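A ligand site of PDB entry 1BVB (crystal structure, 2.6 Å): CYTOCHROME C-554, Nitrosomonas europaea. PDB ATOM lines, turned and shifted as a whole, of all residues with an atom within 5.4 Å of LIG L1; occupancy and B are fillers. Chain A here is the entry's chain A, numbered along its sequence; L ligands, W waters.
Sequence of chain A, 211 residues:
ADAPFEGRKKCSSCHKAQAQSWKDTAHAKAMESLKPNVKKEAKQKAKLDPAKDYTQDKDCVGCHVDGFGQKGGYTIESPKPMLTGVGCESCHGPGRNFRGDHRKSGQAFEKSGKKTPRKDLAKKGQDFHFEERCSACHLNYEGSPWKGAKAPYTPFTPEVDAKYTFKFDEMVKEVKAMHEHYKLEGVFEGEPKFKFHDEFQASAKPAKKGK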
ATOM      1  N   GLY A   7      25.570 -11.216 -29.946  1.00  0.00           N
ATOM      2  CA  GLY A   7      24.592 -11.475 -30.969  1.00  0.00           C
ATOM      3  C   GLY A   7      24.596 -12.944 -31.290  1.00  0.00           C
ATOM      4  O   GLY A   7      25.451 -13.659 -30.848  1.00  0.00           O
ATOM      5  N   LYS A  10      27.895 -16.795 -33.562  1.00  0.00           N
ATOM      6  CA  LYS A  10      28.543 -18.046 -33.258  1.00  0.00           C
ATOM      7  C   LYS A  10      27.637 -19.092 -32.641  1.00  0.00           C
ATOM      8  O   LYS A  10      27.778 -20.273 -32.952  1.00  0.00           O
ATOM      9  CB  LYS A  10      29.749 -17.789 -32.401  1.00  0.00           C
ATOM     10  CG  LYS A  10      30.526 -16.623 -32.967  1.00  0.00           C
ATOM     11  CD  LYS A  10      31.389 -15.981 -31.940  1.00  0.00           C
ATOM     12  CE  LYS A  10      32.820 -15.901 -32.466  1.00  0.00           C
ATOM     13  NZ  LYS A  10      32.961 -15.124 -33.751  1.00  0.00           N
ATOM     14  N   CYS A  11      26.692 -18.682 -31.790  1.00  0.00           N
ATOM     15  CA  CYS A  11      25.782 -19.660 -31.187  1.00  0.00           C
ATOM     16  C   CYS A  11      25.116 -20.422 -32.312  1.00  0.00           C
ATOM     17  O   CYS A  11      25.060 -21.651 -32.273  1.00  0.00           O
ATOM     18  CB  CYS A  11      24.646 -19.009 -30.368  1.00  0.00           C
ATOM     19  SG  CYS A  11      24.996 -17.637 -29.225  1.00  0.00           S
ATOM     20  N   CYS A  14      27.526 -22.971 -34.234  1.00  0.00           N
ATOM     21  CA  CYS A  14      27.722 -24.256 -33.557  1.00  0.00           C
ATOM     22  C   CYS A  14      26.425 -24.964 -33.200  1.00  0.00           C
ATOM     23  O   CYS A  14      26.443 -26.158 -32.922  1.00  0.00           O
ATOM     24  CB  CYS A  14      28.534 -24.095 -32.265  1.00  0.00           C
ATOM     25  SG  CYS A  14      30.255 -23.593 -32.488  1.00  0.00           S
ATOM     26  N   HIS A  15      25.300 -24.242 -33.202  1.00  0.00           N
ATOM     27  CA  HIS A  15      24.006 -24.824 -32.833  1.00  0.00           C
ATOM     28  C   HIS A  15      22.966 -24.595 -33.906  1.00  0.00           C
ATOM     29  O   HIS A  15      21.892 -24.055 -33.629  1.00  0.00           O
ATOM     30  CB  HIS A  15      23.530 -24.226 -31.511  1.00  0.00           C
ATOM     31  CG  HIS A  15      24.419 -24.561 -30.334  1.00  0.00           C
ATOM     32  ND1 HIS A  15      24.681 -25.851 -29.904  1.00  0.00           N
ATOM     33  CD2 HIS A  15      25.083 -23.741 -29.476  1.00  0.00           C
ATOM     34  CE1 HIS A  15      25.472 -25.770 -28.831  1.00  0.00           C
ATOM     35  NE2 HIS A  15      25.739 -24.518 -28.523  1.00  0.00           N
ATOM     36  N   CYS A  88      19.360 -15.798 -28.899  1.00  0.00           N
ATOM     37  CA  CYS A  88      19.977 -16.728 -27.986  1.00  0.00           C
ATOM     38  C   CYS A  88      20.392 -16.173 -26.647  1.00  0.00           C
ATOM     39  O   CYS A  88      20.125 -16.778 -25.614  1.00  0.00           O
ATOM     40  CB  CYS A  88      21.196 -17.358 -28.640  1.00  0.00           C
ATOM     41  SG  CYS A  88      21.055 -17.551 -30.433  1.00  0.00           S
ATOM     42  N   GLU A  89      21.051 -15.020 -26.654  1.00  0.00           N
ATOM     43  CA  GLU A  89      21.481 -14.450 -25.389  1.00  0.00           C
ATOM     44  C   GLU A  89      20.364 -13.845 -24.537  1.00  0.00           C
ATOM     45  O   GLU A  89      20.534 -13.651 -23.361  1.00  0.00           O
ATOM     46  CB  GLU A  89      22.586 -13.409 -25.643  1.00  0.00           C
ATOM     47  CG  GLU A  89      23.782 -14.004 -26.378  1.00  0.00           C
ATOM     48  CD  GLU A  89      24.660 -12.959 -26.992  1.00  0.00           C
ATOM     49  OE1 GLU A  89      24.151 -12.117 -27.757  1.00  0.00           O
ATOM     50  OE2 GLU A  89      25.876 -12.976 -26.707  1.00  0.00           O
ATOM     51  N   HIS A  92      19.806 -17.230 -22.812  1.00  0.00           N
ATOM     52  CA  HIS A  92      21.037 -17.860 -22.326  1.00  0.00           C
ATOM     53  C   HIS A  92      22.126 -16.980 -21.706  1.00  0.00           C
ATOM     54  O   HIS A  92      23.086 -17.479 -21.073  1.00  0.00           O
ATOM     55  CB  HIS A  92      21.630 -18.669 -23.442  1.00  0.00           C
ATOM     56  CG  HIS A  92      20.752 -19.785 -23.861  1.00  0.00           C
ATOM     57  ND1 HIS A  92      20.604 -20.955 -23.151  1.00  0.00           N
ATOM     58  CD2 HIS A  92      19.919 -19.892 -24.934  1.00  0.00           C
ATOM     59  CE1 HIS A  92      19.719 -21.715 -23.818  1.00  0.00           C
ATOM     60  NE2 HIS A  92      19.272 -21.110 -24.901  1.00  0.00           N
ATOM     61  N   GLY A  93      21.961 -15.683 -21.898  1.00  0.00           N
ATOM     62  CA  GLY A  93      22.845 -14.714 -21.307  1.00  0.00           C
ATOM     63  C   GLY A  93      23.899 -14.247 -22.263  1.00  0.00           C
ATOM     64  O   GLY A  93      24.169 -14.903 -23.254  1.00  0.00           O
ATOM     65  N   GLY A  95      27.121 -13.963 -24.101  1.00  0.00           N
ATOM     66  CA  GLY A  95      28.088 -15.054 -24.153  1.00  0.00           C
ATOM     67  C   GLY A  95      29.519 -14.782 -24.577  1.00  0.00           C
ATOM     68  O   GLY A  95      30.239 -15.709 -24.972  1.00  0.00           O
ATOM     69  N   PHE A  98      31.426 -17.012 -22.189  1.00  0.00           N
ATOM     70  CA  PHE A  98      31.198 -18.413 -21.989  1.00  0.00           C
ATOM     71  C   PHE A  98      31.245 -19.273 -23.223  1.00  0.00           C
ATOM     72  O   PHE A  98      31.413 -20.474 -23.118  1.00  0.00           O
ATOM     73  CB  PHE A  98      29.900 -18.629 -21.206  1.00  0.00           C
ATOM     74  CG  PHE A  98      28.626 -18.382 -21.999  1.00  0.00           C
ATOM     75  CD1 PHE A  98      28.303 -19.167 -23.110  1.00  0.00           C
ATOM     76  CD2 PHE A  98      27.676 -17.450 -21.543  1.00  0.00           C
ATOM     77  CE1 PHE A  98      27.039 -19.036 -23.750  1.00  0.00           C
ATOM     78  CE2 PHE A  98      26.421 -17.316 -22.172  1.00  0.00           C
ATOM     79  CZ  PHE A  98      26.105 -18.107 -23.278  1.00  0.00           C
ATOM     80  N   ARG A  99      31.113 -18.683 -24.388  1.00  0.00           N
ATOM     81  CA  ARG A  99      31.133 -19.525 -25.583  1.00  0.00           C
ATOM     82  C   ARG A  99      32.534 -20.062 -25.771  1.00  0.00           C
ATOM     83  O   ARG A  99      32.725 -21.122 -26.373  1.00  0.00           O
ATOM     84  CB  ARG A  99      30.710 -18.749 -26.820  1.00  0.00           C
ATOM     85  CG  ARG A  99      31.509 -17.512 -27.067  1.00  0.00           C
ATOM     86  CD  ARG A  99      31.150 -16.930 -28.407  1.00  0.00           C
ATOM     87  NE  ARG A  99      31.942 -15.751 -28.679  1.00  0.00           N
ATOM     88  CZ  ARG A  99      33.132 -15.793 -29.272  1.00  0.00           C
ATOM     89  NH1 ARG A  99      33.618 -16.968 -29.629  1.00  0.00           N
ATOM     90  NH2 ARG A  99      33.828 -14.692 -29.460  1.00  0.00           N
ATOM     91  N   HIS A 102      32.545 -23.293 -24.476  1.00  0.00           N
ATOM     92  CA  HIS A 102      31.752 -24.246 -25.249  1.00  0.00           C
ATOM     93  C   HIS A 102      32.626 -24.887 -26.319  1.00  0.00           C
ATOM     94  O   HIS A 102      32.429 -26.036 -26.666  1.00  0.00           O
ATOM     95  CB  HIS A 102      30.562 -23.572 -25.914  1.00  0.00           C
ATOM     96  CG  HIS A 102      29.483 -23.164 -24.969  1.00  0.00           C
ATOM     97  ND1 HIS A 102      28.169 -23.169 -25.332  1.00  0.00           N
ATOM     98  CD2 HIS A 102      29.590 -22.779 -23.673  1.00  0.00           C
ATOM     99  CE1 HIS A 102      27.506 -22.786 -24.257  1.00  0.00           C
ATOM    100  NE2 HIS A 102      28.329 -22.541 -23.228  1.00  0.00           N
ATOM    101  N   ARG A 103      33.574 -24.138 -26.840  1.00  0.00           N
ATOM    102  CA  ARG A 103      34.454 -24.681 -27.868  1.00  0.00           C
ATOM    103  C   ARG A 103      35.442 -25.648 -27.220  1.00  0.00           C
ATOM    104  O   ARG A 103      35.436 -26.855 -27.527  1.00  0.00           O
ATOM    105  CB  ARG A 103      35.229 -23.567 -28.569  1.00  0.00           C
ATOM    106  CG  ARG A 103      35.742 -23.971 -29.938  1.00  0.00           C
ATOM    107  CD  ARG A 103      36.483 -22.823 -30.614  1.00  0.00           C
ATOM    108  NE  ARG A 103      37.076 -23.255 -31.883  1.00  0.00           N
ATOM    109  CZ  ARG A 103      38.326 -23.693 -32.027  1.00  0.00           C
ATOM    110  NH1 ARG A 103      39.138 -23.767 -30.966  1.00  0.00           N
ATOM    111  NH2 ARG A 103      38.774 -24.071 -33.217  1.00  0.00           N
ATOM    112  N   GLY A 106      34.032 -28.806 -25.900  1.00  0.00           N
ATOM    113  CA  GLY A 106      33.544 -29.643 -26.980  1.00  0.00           C
ATOM    114  C   GLY A 106      34.677 -30.505 -27.500  1.00  0.00           C
ATOM    115  O   GLY A 106      34.534 -31.711 -27.644  1.00  0.00           O
ATOM    116  N   ARG A 118      28.931 -27.251 -15.217  1.00  0.00           N
ATOM    117  CA  ARG A 118      28.166 -26.073 -15.614  1.00  0.00           C
ATOM    118  C   ARG A 118      28.598 -24.870 -14.777  1.00  0.00           C
ATOM    119  O   ARG A 118      28.477 -23.712 -15.202  1.00  0.00           O
ATOM    120  CB  ARG A 118      26.665 -26.295 -15.417  1.00  0.00           C
ATOM    121  CG  ARG A 118      26.024 -27.229 -16.405  1.00  0.00           C
ATOM    122  CD  ARG A 118      24.539 -27.047 -16.405  1.00  0.00           C
ATOM    123  NE  ARG A 118      23.910 -27.844 -17.450  1.00  0.00           N
ATOM    124  CZ  ARG A 118      23.657 -29.144 -17.328  1.00  0.00           C
ATOM    125  NH1 ARG A 118      23.994 -29.751 -16.195  1.00  0.00           N
ATOM    126  NH2 ARG A 118      23.091 -29.827 -18.322  1.00  0.00           N
ATOM    127  N   LEU A 121      30.555 -22.425 -16.582  1.00  0.00           N
ATOM    128  CA  LEU A 121      29.784 -21.658 -17.550  1.00  0.00           C
ATOM    129  C   LEU A 121      28.966 -20.607 -16.803  1.00  0.00           C
ATOM    130  O   LEU A 121      28.945 -19.440 -17.212  1.00  0.00           O
ATOM    131  CB  LEU A 121      28.873 -22.584 -18.361  1.00  0.00           C
ATOM    132  CG  LEU A 121      29.500 -23.731 -19.147  1.00  0.00           C
ATOM    133  CD1 LEU A 121      28.407 -24.605 -19.731  1.00  0.00           C
ATOM    134  CD2 LEU A 121      30.359 -23.175 -20.278  1.00  0.00           C
ATOM    135  N   GLN A 126      26.763 -17.749 -18.184  1.00  0.00           N
ATOM    136  CA  GLN A 126      25.678 -18.452 -18.832  1.00  0.00           C
ATOM    137  C   GLN A 126      24.495 -18.585 -17.878  1.00  0.00           C
ATOM    138  O   GLN A 126      24.678 -18.786 -16.676  1.00  0.00           O
ATOM    139  CB  GLN A 126      26.112 -19.814 -19.310  1.00  0.00           C
ATOM    140  CG  GLN A 126      25.044 -20.468 -20.157  1.00  0.00           C
ATOM    141  CD  GLN A 126      25.608 -21.514 -21.064  1.00  0.00           C
ATOM    142  OE1 GLN A 126      26.835 -21.554 -21.192  1.00  0.00           O
ATOM    143  NE2 GLN A 126      24.822 -22.286 -21.648  1.00  0.00           N
ATOM    144  N   PHE A 128      21.193 -20.569 -16.579  1.00  0.00           N
ATOM    145  CA  PHE A 128      20.559 -21.884 -16.531  1.00  0.00           C
ATOM    146  C   PHE A 128      19.234 -21.836 -15.750  1.00  0.00           C
ATOM    147  O   PHE A 128      18.796 -22.873 -15.231  1.00  0.00           O
ATOM    148  CB  PHE A 128      21.495 -22.882 -15.849  1.00  0.00           C
ATOM    149  CG  PHE A 128      22.789 -23.104 -16.575  1.00  0.00           C
ATOM    150  CD1 PHE A 128      22.859 -24.008 -17.630  1.00  0.00           C
ATOM    151  CD2 PHE A 128      23.948 -22.431 -16.188  1.00  0.00           C
ATOM    152  CE1 PHE A 128      24.066 -24.236 -18.303  1.00  0.00           C
ATOM    153  CE2 PHE A 128      25.148 -22.657 -16.849  1.00  0.00           C
ATOM    154  CZ  PHE A 128      25.210 -23.564 -17.916  1.00  0.00           C
ATOM    155  N   LYS A 183      19.112 -33.544 -28.851  1.00  0.00           N
ATOM    156  CA  LYS A 183      19.989 -34.340 -28.001  1.00  0.00           C
ATOM    157  C   LYS A 183      21.428 -33.898 -27.787  1.00  0.00           C
ATOM    158  O   LYS A 183      22.210 -33.674 -28.724  1.00  0.00           O
ATOM    159  CB  LYS A 183      20.003 -35.794 -28.455  1.00  0.00           C
ATOM    160  CG  LYS A 183      18.799 -36.580 -27.958  1.00  0.00           C
ATOM    161  CD  LYS A 183      18.692 -36.576 -26.439  1.00  0.00           C
ATOM    162  CE  LYS A 183      18.119 -37.888 -25.899  1.00  0.00           C
ATOM    163  NZ  LYS A 183      16.716 -38.081 -26.321  1.00  0.00           N
ATOM    164  N   LEU A 184      21.787 -33.815 -26.514  1.00  0.00           N
ATOM    165  CA  LEU A 184      23.102 -33.436 -26.111  1.00  0.00           C
ATOM    166  C   LEU A 184      23.858 -34.699 -25.783  1.00  0.00           C
ATOM    167  O   LEU A 184      23.268 -35.694 -25.362  1.00  0.00           O
ATOM    168  CB  LEU A 184      23.030 -32.498 -24.887  1.00  0.00           C
ATOM    169  CG  LEU A 184      22.379 -31.143 -25.170  1.00  0.00           C
ATOM    170  CD1 LEU A 184      21.911 -30.503 -23.907  1.00  0.00           C
ATOM    171  CD2 LEU A 184      23.403 -30.284 -25.841  1.00  0.00           C
ATOM    172  N   GLU A 185      25.166 -34.668 -26.019  1.00  0.00           N
ATOM    173  CA  GLU A 185      26.033 -35.785 -25.734  1.00  0.00           C
ATOM    174  C   GLU A 185      26.427 -35.625 -24.265  1.00  0.00           C
ATOM    175  O   GLU A 185      26.874 -36.574 -23.633  1.00  0.00           O
ATOM    176  CB  GLU A 185      27.238 -35.734 -26.631  1.00  0.00           C
ATOM    177  CG  GLU A 185      26.871 -35.813 -28.084  1.00  0.00           C
ATOM    178  CD  GLU A 185      27.964 -36.451 -28.886  1.00  0.00           C
ATOM    179  OE1 GLU A 185      28.191 -37.670 -28.677  1.00  0.00           O
ATOM    180  OE2 GLU A 185      28.583 -35.746 -29.730  1.00  0.00           O
ATOM    181  N   GLY A 186      26.244 -34.417 -23.749  1.00  0.00           N
ATOM    182  CA  GLY A 186      26.506 -34.156 -22.354  1.00  0.00           C
ATOM    183  C   GLY A 186      27.929 -33.790 -22.016  1.00  0.00           C
ATOM    184  O   GLY A 186      28.505 -34.400 -21.091  1.00  0.00           O
ATOM    185  N   VAL A 187      28.497 -32.820 -22.731  1.00  0.00           N
ATOM    186  CA  VAL A 187      29.853 -32.415 -22.416  1.00  0.00           C
ATOM    187  C   VAL A 187      29.841 -31.596 -21.126  1.00  0.00           C
ATOM    188  O   VAL A 187      30.852 -31.541 -20.427  1.00  0.00           O
ATOM    189  CB  VAL A 187      30.557 -31.629 -23.584  1.00  0.00           C
ATOM    190  CG1 VAL A 187      29.862 -31.870 -24.869  1.00  0.00           C
ATOM    191  CG2 VAL A 187      30.674 -30.177 -23.264  1.00  0.00           C
ATOM    192  N   PHE A 188      28.684 -31.016 -20.801  1.00  0.00           N
ATOM    193  CA  PHE A 188      28.532 -30.227 -19.590  1.00  0.00           C
ATOM    194  C   PHE A 188      27.609 -30.986 -18.663  1.00  0.00           C
ATOM    195  O   PHE A 188      26.643 -31.633 -19.127  1.00  0.00           O
ATOM    196  CB  PHE A 188      27.949 -28.856 -19.906  1.00  0.00           C
ATOM    197  CG  PHE A 188      28.871 -27.966 -20.681  1.00  0.00           C
ATOM    198  CD1 PHE A 188      30.059 -27.517 -20.129  1.00  0.00           C
ATOM    199  CD2 PHE A 188      28.602 -27.649 -22.018  1.00  0.00           C
ATOM    200  CE1 PHE A 188      30.975 -26.787 -20.878  1.00  0.00           C
ATOM    201  CE2 PHE A 188      29.503 -26.910 -22.776  1.00  0.00           C
ATOM    202  CZ  PHE A 188      30.693 -26.488 -22.211  1.00  0.00           C
ATOM    203  N   HIS A 197      15.607 -29.622 -17.497  1.00  0.00           N
ATOM    204  CA  HIS A 197      16.640 -30.056 -18.411  1.00  0.00           C
ATOM    205  C   HIS A 197      16.565 -31.538 -18.745  1.00  0.00           C
ATOM    206  O   HIS A 197      16.602 -31.915 -19.923  1.00  0.00           O
ATOM    207  CB  HIS A 197      18.012 -29.731 -17.852  1.00  0.00           C
ATOM    208  CG  HIS A 197      19.127 -30.213 -18.733  1.00  0.00           C
ATOM    209  ND1 HIS A 197      19.556 -29.512 -19.831  1.00  0.00           N
ATOM    210  CD2 HIS A 197      19.862 -31.349 -18.702  1.00  0.00           C
ATOM    211  CE1 HIS A 197      20.525 -30.182 -20.433  1.00  0.00           C
ATOM    212  NE2 HIS A 197      20.720 -31.305 -19.769  1.00  0.00           N
ATOM    213  N   LYS A 211      29.759 -30.342 -35.703  1.00  0.00           N
ATOM    214  CA  LYS A 211      30.382 -29.664 -34.545  1.00  0.00           C
ATOM    215  C   LYS A 211      31.919 -29.683 -34.603  1.00  0.00           C
ATOM    216  O   LYS A 211      32.526 -28.586 -34.667  1.00  0.00           O
ATOM    217  CB  LYS A 211      29.919 -30.304 -33.220  1.00  0.00           C
ATOM    218  CG  LYS A 211      30.523 -29.666 -31.961  1.00  0.00           C
ATOM    219  CD  LYS A 211      30.023 -28.236 -31.743  1.00  0.00           C
ATOM    220  CE  LYS A 211      31.161 -27.341 -31.301  1.00  0.00           C
ATOM    221  NZ  LYS A 211      32.244 -27.295 -32.305  1.00  0.00           N
ATOM    222  OXT LYS A 211      32.503 -30.793 -34.579  1.00  0.00           O
HETATM  223  C1  LIG L   1      26.247 -26.689 -25.392  1.00  0.00           C
HETATM  224  C2  LIG L   1      24.268 -22.290 -25.690  1.00  0.00           C
HETATM  225  C3  LIG L   1      27.842 -20.924 -28.561  1.00  0.00           C
HETATM  226  C4  LIG L   1      29.471 -25.462 -28.732  1.00  0.00           C
HETATM  227  C5  LIG L   1      25.420 -25.592 -25.175  1.00  0.00           C
HETATM  228  C6  LIG L   1      24.262 -25.602 -24.294  1.00  0.00           C
HETATM  229  C7  LIG L   1      23.690 -24.387 -24.387  1.00  0.00           C
HETATM  230  C8  LIG L   1      24.511 -23.619 -25.333  1.00  0.00           C
HETATM  231  C9  LIG L   1      22.436 -23.923 -23.642  1.00  0.00           C
HETATM  232  C10 LIG L   1      23.792 -26.735 -23.422  1.00  0.00           C
HETATM  233  C11 LIG L   1      24.452 -26.685 -22.050  1.00  0.00           C
HETATM  234  C12 LIG L   1      23.764 -27.563 -21.019  1.00  0.00           C
HETATM  235  O1  LIG L   1      23.902 -28.816 -21.135  1.00  0.00           O
HETATM  236  O2  LIG L   1      23.089 -27.000 -20.077  1.00  0.00           O
HETATM  237  C13 LIG L   1      25.048 -21.534 -26.535  1.00  0.00           C
HETATM  238  C14 LIG L   1      24.821 -20.117 -26.811  1.00  0.00           C
HETATM  239  C15 LIG L   1      25.895 -19.697 -27.540  1.00  0.00           C
HETATM  240  C16 LIG L   1      26.726 -20.894 -27.754  1.00  0.00           C
HETATM  241  C17 LIG L   1      23.629 -19.244 -26.401  1.00  0.00           C
HETATM  242  C18 LIG L   1      26.214 -18.294 -28.110  1.00  0.00           C
HETATM  243  C19 LIG L   1      26.493 -17.255 -27.048  1.00  0.00           C
HETATM  244  C20 LIG L   1      28.570 -22.048 -28.878  1.00  0.00           C
HETATM  245  C21 LIG L   1      29.645 -22.051 -29.830  1.00  0.00           C
HETATM  246  C22 LIG L   1      30.049 -23.305 -29.910  1.00  0.00           C
HETATM  247  C23 LIG L   1      29.283 -24.092 -28.988  1.00  0.00           C
HETATM  248  C24 LIG L   1      30.197 -20.880 -30.628  1.00  0.00           C
HETATM  249  C25 LIG L   1      31.111 -23.816 -30.861  1.00  0.00           C
HETATM  250  C26 LIG L   1      32.472 -23.112 -30.938  1.00  0.00           C
HETATM  251  C27 LIG L   1      28.746 -26.192 -27.800  1.00  0.00           C
HETATM  252  C28 LIG L   1      28.989 -27.589 -27.488  1.00  0.00           C
HETATM  253  C29 LIG L   1      28.066 -27.919 -26.508  1.00  0.00           C
HETATM  254  C30 LIG L   1      27.303 -26.739 -26.250  1.00  0.00           C
HETATM  255  C31 LIG L   1      30.024 -28.541 -28.130  1.00  0.00           C
HETATM  256  C32 LIG L   1      27.944 -29.321 -25.960  1.00  0.00           C
HETATM  257  C33 LIG L   1      27.095 -30.290 -26.741  1.00  0.00           C
HETATM  258  C34 LIG L   1      26.687 -31.544 -26.050  1.00  0.00           C
HETATM  259  O3  LIG L   1      26.065 -32.363 -26.736  1.00  0.00           O
HETATM  260  O4  LIG L   1      26.968 -31.719 -24.835  1.00  0.00           O
HETATM  261  N1  LIG L   1      25.573 -24.369 -25.797  1.00  0.00           N
HETATM  262  N2  LIG L   1      26.208 -22.019 -27.122  1.00  0.00           N
HETATM  263  N3  LIG L   1      28.339 -23.299 -28.371  1.00  0.00           N
HETATM  264  N4  LIG L   1      27.718 -25.657 -27.036  1.00  0.00           N
HETATM  265 FE1  LIG L   1      26.989 -23.825 -27.065  1.00  0.00          FE
HETATM  266  C1  LG2 L   2      18.281 -24.937 -24.592  1.00  0.00           C
HETATM  267  C2  LG2 L   2      20.721 -22.963 -28.265  1.00  0.00           C
HETATM  268  C3  LG2 L   2      17.730 -19.172 -28.145  1.00  0.00           C
HETATM  269  C4  LG2 L   2      15.485 -21.021 -24.261  1.00  0.00           C
HETATM  270  C5  LG2 L   2      19.199 -24.738 -25.608  1.00  0.00           C
HETATM  271  C6  LG2 L   2      20.251 -25.694 -25.953  1.00  0.00           C
HETATM  272  C7  LG2 L   2      20.962 -25.150 -26.980  1.00  0.00           C
HETATM  273  C8  LG2 L   2      20.313 -23.843 -27.270  1.00  0.00           C
HETATM  274  C9  LG2 L   2      22.157 -25.782 -27.661  1.00  0.00           C
HETATM  275  C10 LG2 L   2      20.497 -27.021 -25.292  1.00  0.00           C
HETATM  276  C11 LG2 L   2      19.991 -28.238 -26.085  1.00  0.00           C
HETATM  277  C12 LG2 L   2      18.551 -28.148 -26.558  1.00  0.00           C
HETATM  278  O1  LG2 L   2      17.629 -28.112 -25.719  1.00  0.00           O
HETATM  279  O2  LG2 L   2      18.346 -28.118 -27.782  1.00  0.00           O
HETATM  280  C13 LG2 L   2      20.119 -21.754 -28.555  1.00  0.00           C
HETATM  281  C14 LG2 L   2      20.528 -20.883 -29.627  1.00  0.00           C
HETATM  282  C15 LG2 L   2      19.663 -19.817 -29.640  1.00  0.00           C
HETATM  283  C16 LG2 L   2      18.739 -20.045 -28.534  1.00  0.00           C
HETATM  284  C17 LG2 L   2      21.719 -21.117 -30.586  1.00  0.00           C
HETATM  285  C18 LG2 L   2      19.642 -18.616 -30.583  1.00  0.00           C
HETATM  286  C19 LG2 L   2      19.457 -18.968 -32.043  1.00  0.00           C
HETATM  287  C20 LG2 L   2      16.858 -19.347 -27.054  1.00  0.00           C
HETATM  288  C21 LG2 L   2      15.861 -18.355 -26.632  1.00  0.00           C
HETATM  289  C22 LG2 L   2      15.280 -18.869 -25.554  1.00  0.00           C
HETATM  290  C23 LG2 L   2      15.876 -20.168 -25.300  1.00  0.00           C
HETATM  291  C24 LG2 L   2      15.564 -16.994 -27.284  1.00  0.00           C
HETATM  292  C25 LG2 L   2      14.232 -18.211 -24.701  1.00  0.00           C
HETATM  293  C26 LG2 L   2      12.937 -17.708 -25.357  1.00  0.00           C
HETATM  294  C27 LG2 L   2      16.041 -22.264 -24.036  1.00  0.00           C
HETATM  295  C28 LG2 L   2      15.618 -23.166 -22.973  1.00  0.00           C
HETATM  296  C29 LG2 L   2      16.404 -24.275 -23.088  1.00  0.00           C
HETATM  297  C30 LG2 L   2      17.285 -24.039 -24.201  1.00  0.00           C
HETATM  298  C31 LG2 L   2      14.521 -22.936 -21.912  1.00  0.00           C
HETATM  299  C32 LG2 L   2      16.457 -25.397 -22.055  1.00  0.00           C
HETATM  300  C33 LG2 L   2      17.640 -25.379 -21.089  1.00  0.00           C
HETATM  301  C34 LG2 L   2      18.132 -26.720 -20.568  1.00  0.00           C
HETATM  302  O3  LG2 L   2      19.190 -26.755 -19.862  1.00  0.00           O
HETATM  303  O4  LG2 L   2      17.467 -27.732 -20.827  1.00  0.00           O
HETATM  304  N1  LG2 L   2      19.241 -23.607 -26.420  1.00  0.00           N
HETATM  305  N2  LG2 L   2      19.008 -21.240 -27.868  1.00  0.00           N
HETATM  306  N3  LG2 L   2      16.866 -20.449 -26.230  1.00  0.00           N
HETATM  307  N4  LG2 L   2      17.055 -22.799 -24.800  1.00  0.00           N
HETATM  308 FE1  LG2 L   2      18.013 -22.032 -26.349  1.00  0.00          FE
HETATM  309  O   HOH W   1      21.327 -25.022 -20.506  1.00  0.00           O
HETATM  310  O   HOH W   2      21.759 -22.245 -20.761  1.00  0.00           O
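An oxygen (O2) of LIG L1 is in salt-bridge range of the guanidinium group (NE) of Arg 118 (2.9 Å). N of Val 187 is in hydrogen-bond range of O4 of LIG L1 (2.8 Å). SG of Cys 11 is covalently linked to C18 of LIG L1, at 1.8 Å. NE2 of His 15 is bound to FE1 of LIG L1. N of Gly 186 is in hydrogen-bond range of O4 of LIG L1 (3.0 Å). The backbone NH (N) of Glu 185 is in hydrogen-bond range of an oxygen (O3) of LIG L1, 2.6 Å away. A carbon (C18) of LG2 L2 is bonded to the side-chain sulfur of Cys 88 (1.8 Å). SG of Cys 14 is bonded to C25 of LIG L1, 1.9 Å away. ND1 of His 197 is in hydrogen-bond range of O3 of LG2 L2, at 2.8 Å. An iron atom (FE1) of LIG L1 is bound by a ring nitrogen (ND1) of His 102 (2.2 Å). A ring nitrogen (NE2) of His 92 is bound to an iron atom (FE1) of LG2 L2 (2.1 Å).
A ring nitrogen (NE2) of His 102 sits at hydrogen-bond distance from the side-chain amide oxygen (OE1) of Gln 126 (2.7 Å). NE2 of His 197 lies within hydrogen-bond range of NH2 of Arg 118. The backbone NH (N) of Gly 95 is in hydrogen-bond range of the side-chain carboxylate (OE2) of Glu 89. The backbone NH (N) of Gln 126 lies within hydrogen-bond range of the backbone carbonyl oxygen (O) of Leu 121 (2.9 Å).
Lys 10 touches LIG L1. Cys 88 touches LIG L1 (CB to C17, 3.8 Å). His 92 touches LIG L1 (CE1 to C9, 3.5 Å). Gly 95 touches LIG L1. CE1 of Phe 98 touches C19 of LIG L1, 3.8 Å away. Arg 99 touches LIG L1. CG of Arg 103 touches C26 of LIG L1, 3.5 Å away. Gly 106 touches LIG L1 (CA to C31, 3.9 Å). NE2 of Gln 126 touches C9 of LIG L1, at 3.5 Å. Phe 128 touches LIG L1. Leu 184 touches LIG L1. His 197 touches LIG L1. CE of Lys 211 touches C25 of LIG L1, at 3.6 Å. Hydrophobic or aromatic side chains within 4 Å of LIG L1: His 15, His 92, Phe 98, His 102, Phe 128, Leu 184, Val 187 and His 197. Within 4 Å of LIG L1: Lys 10, Cys 11, Cys 14, His 15, Cys 88, His 92, Gly 95, Phe 98, Arg 99, His 102, Arg 103, Gly 106, Arg 118, Gln 126, Phe 128, Leu 184, Glu 185, Gly 186, Val 187, His 197 and Lys 211. Along chain A the residues within 4 Å of LIG L1 span positions 10 to 211. The nearest printed residue that does not touch LIG L1 is Phe 188 (4.1 Å).
Water W1 bridges O2 of LIG L1 (2.7 Å) and O3 of LG2 L2 (2.8 Å). Water W2 lies within hydrogen-bond range of a ring nitrogen (ND1) of His 92 (3.0 Å) and the side-chain amide nitrogen of Gln 126 (3.2 Å).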
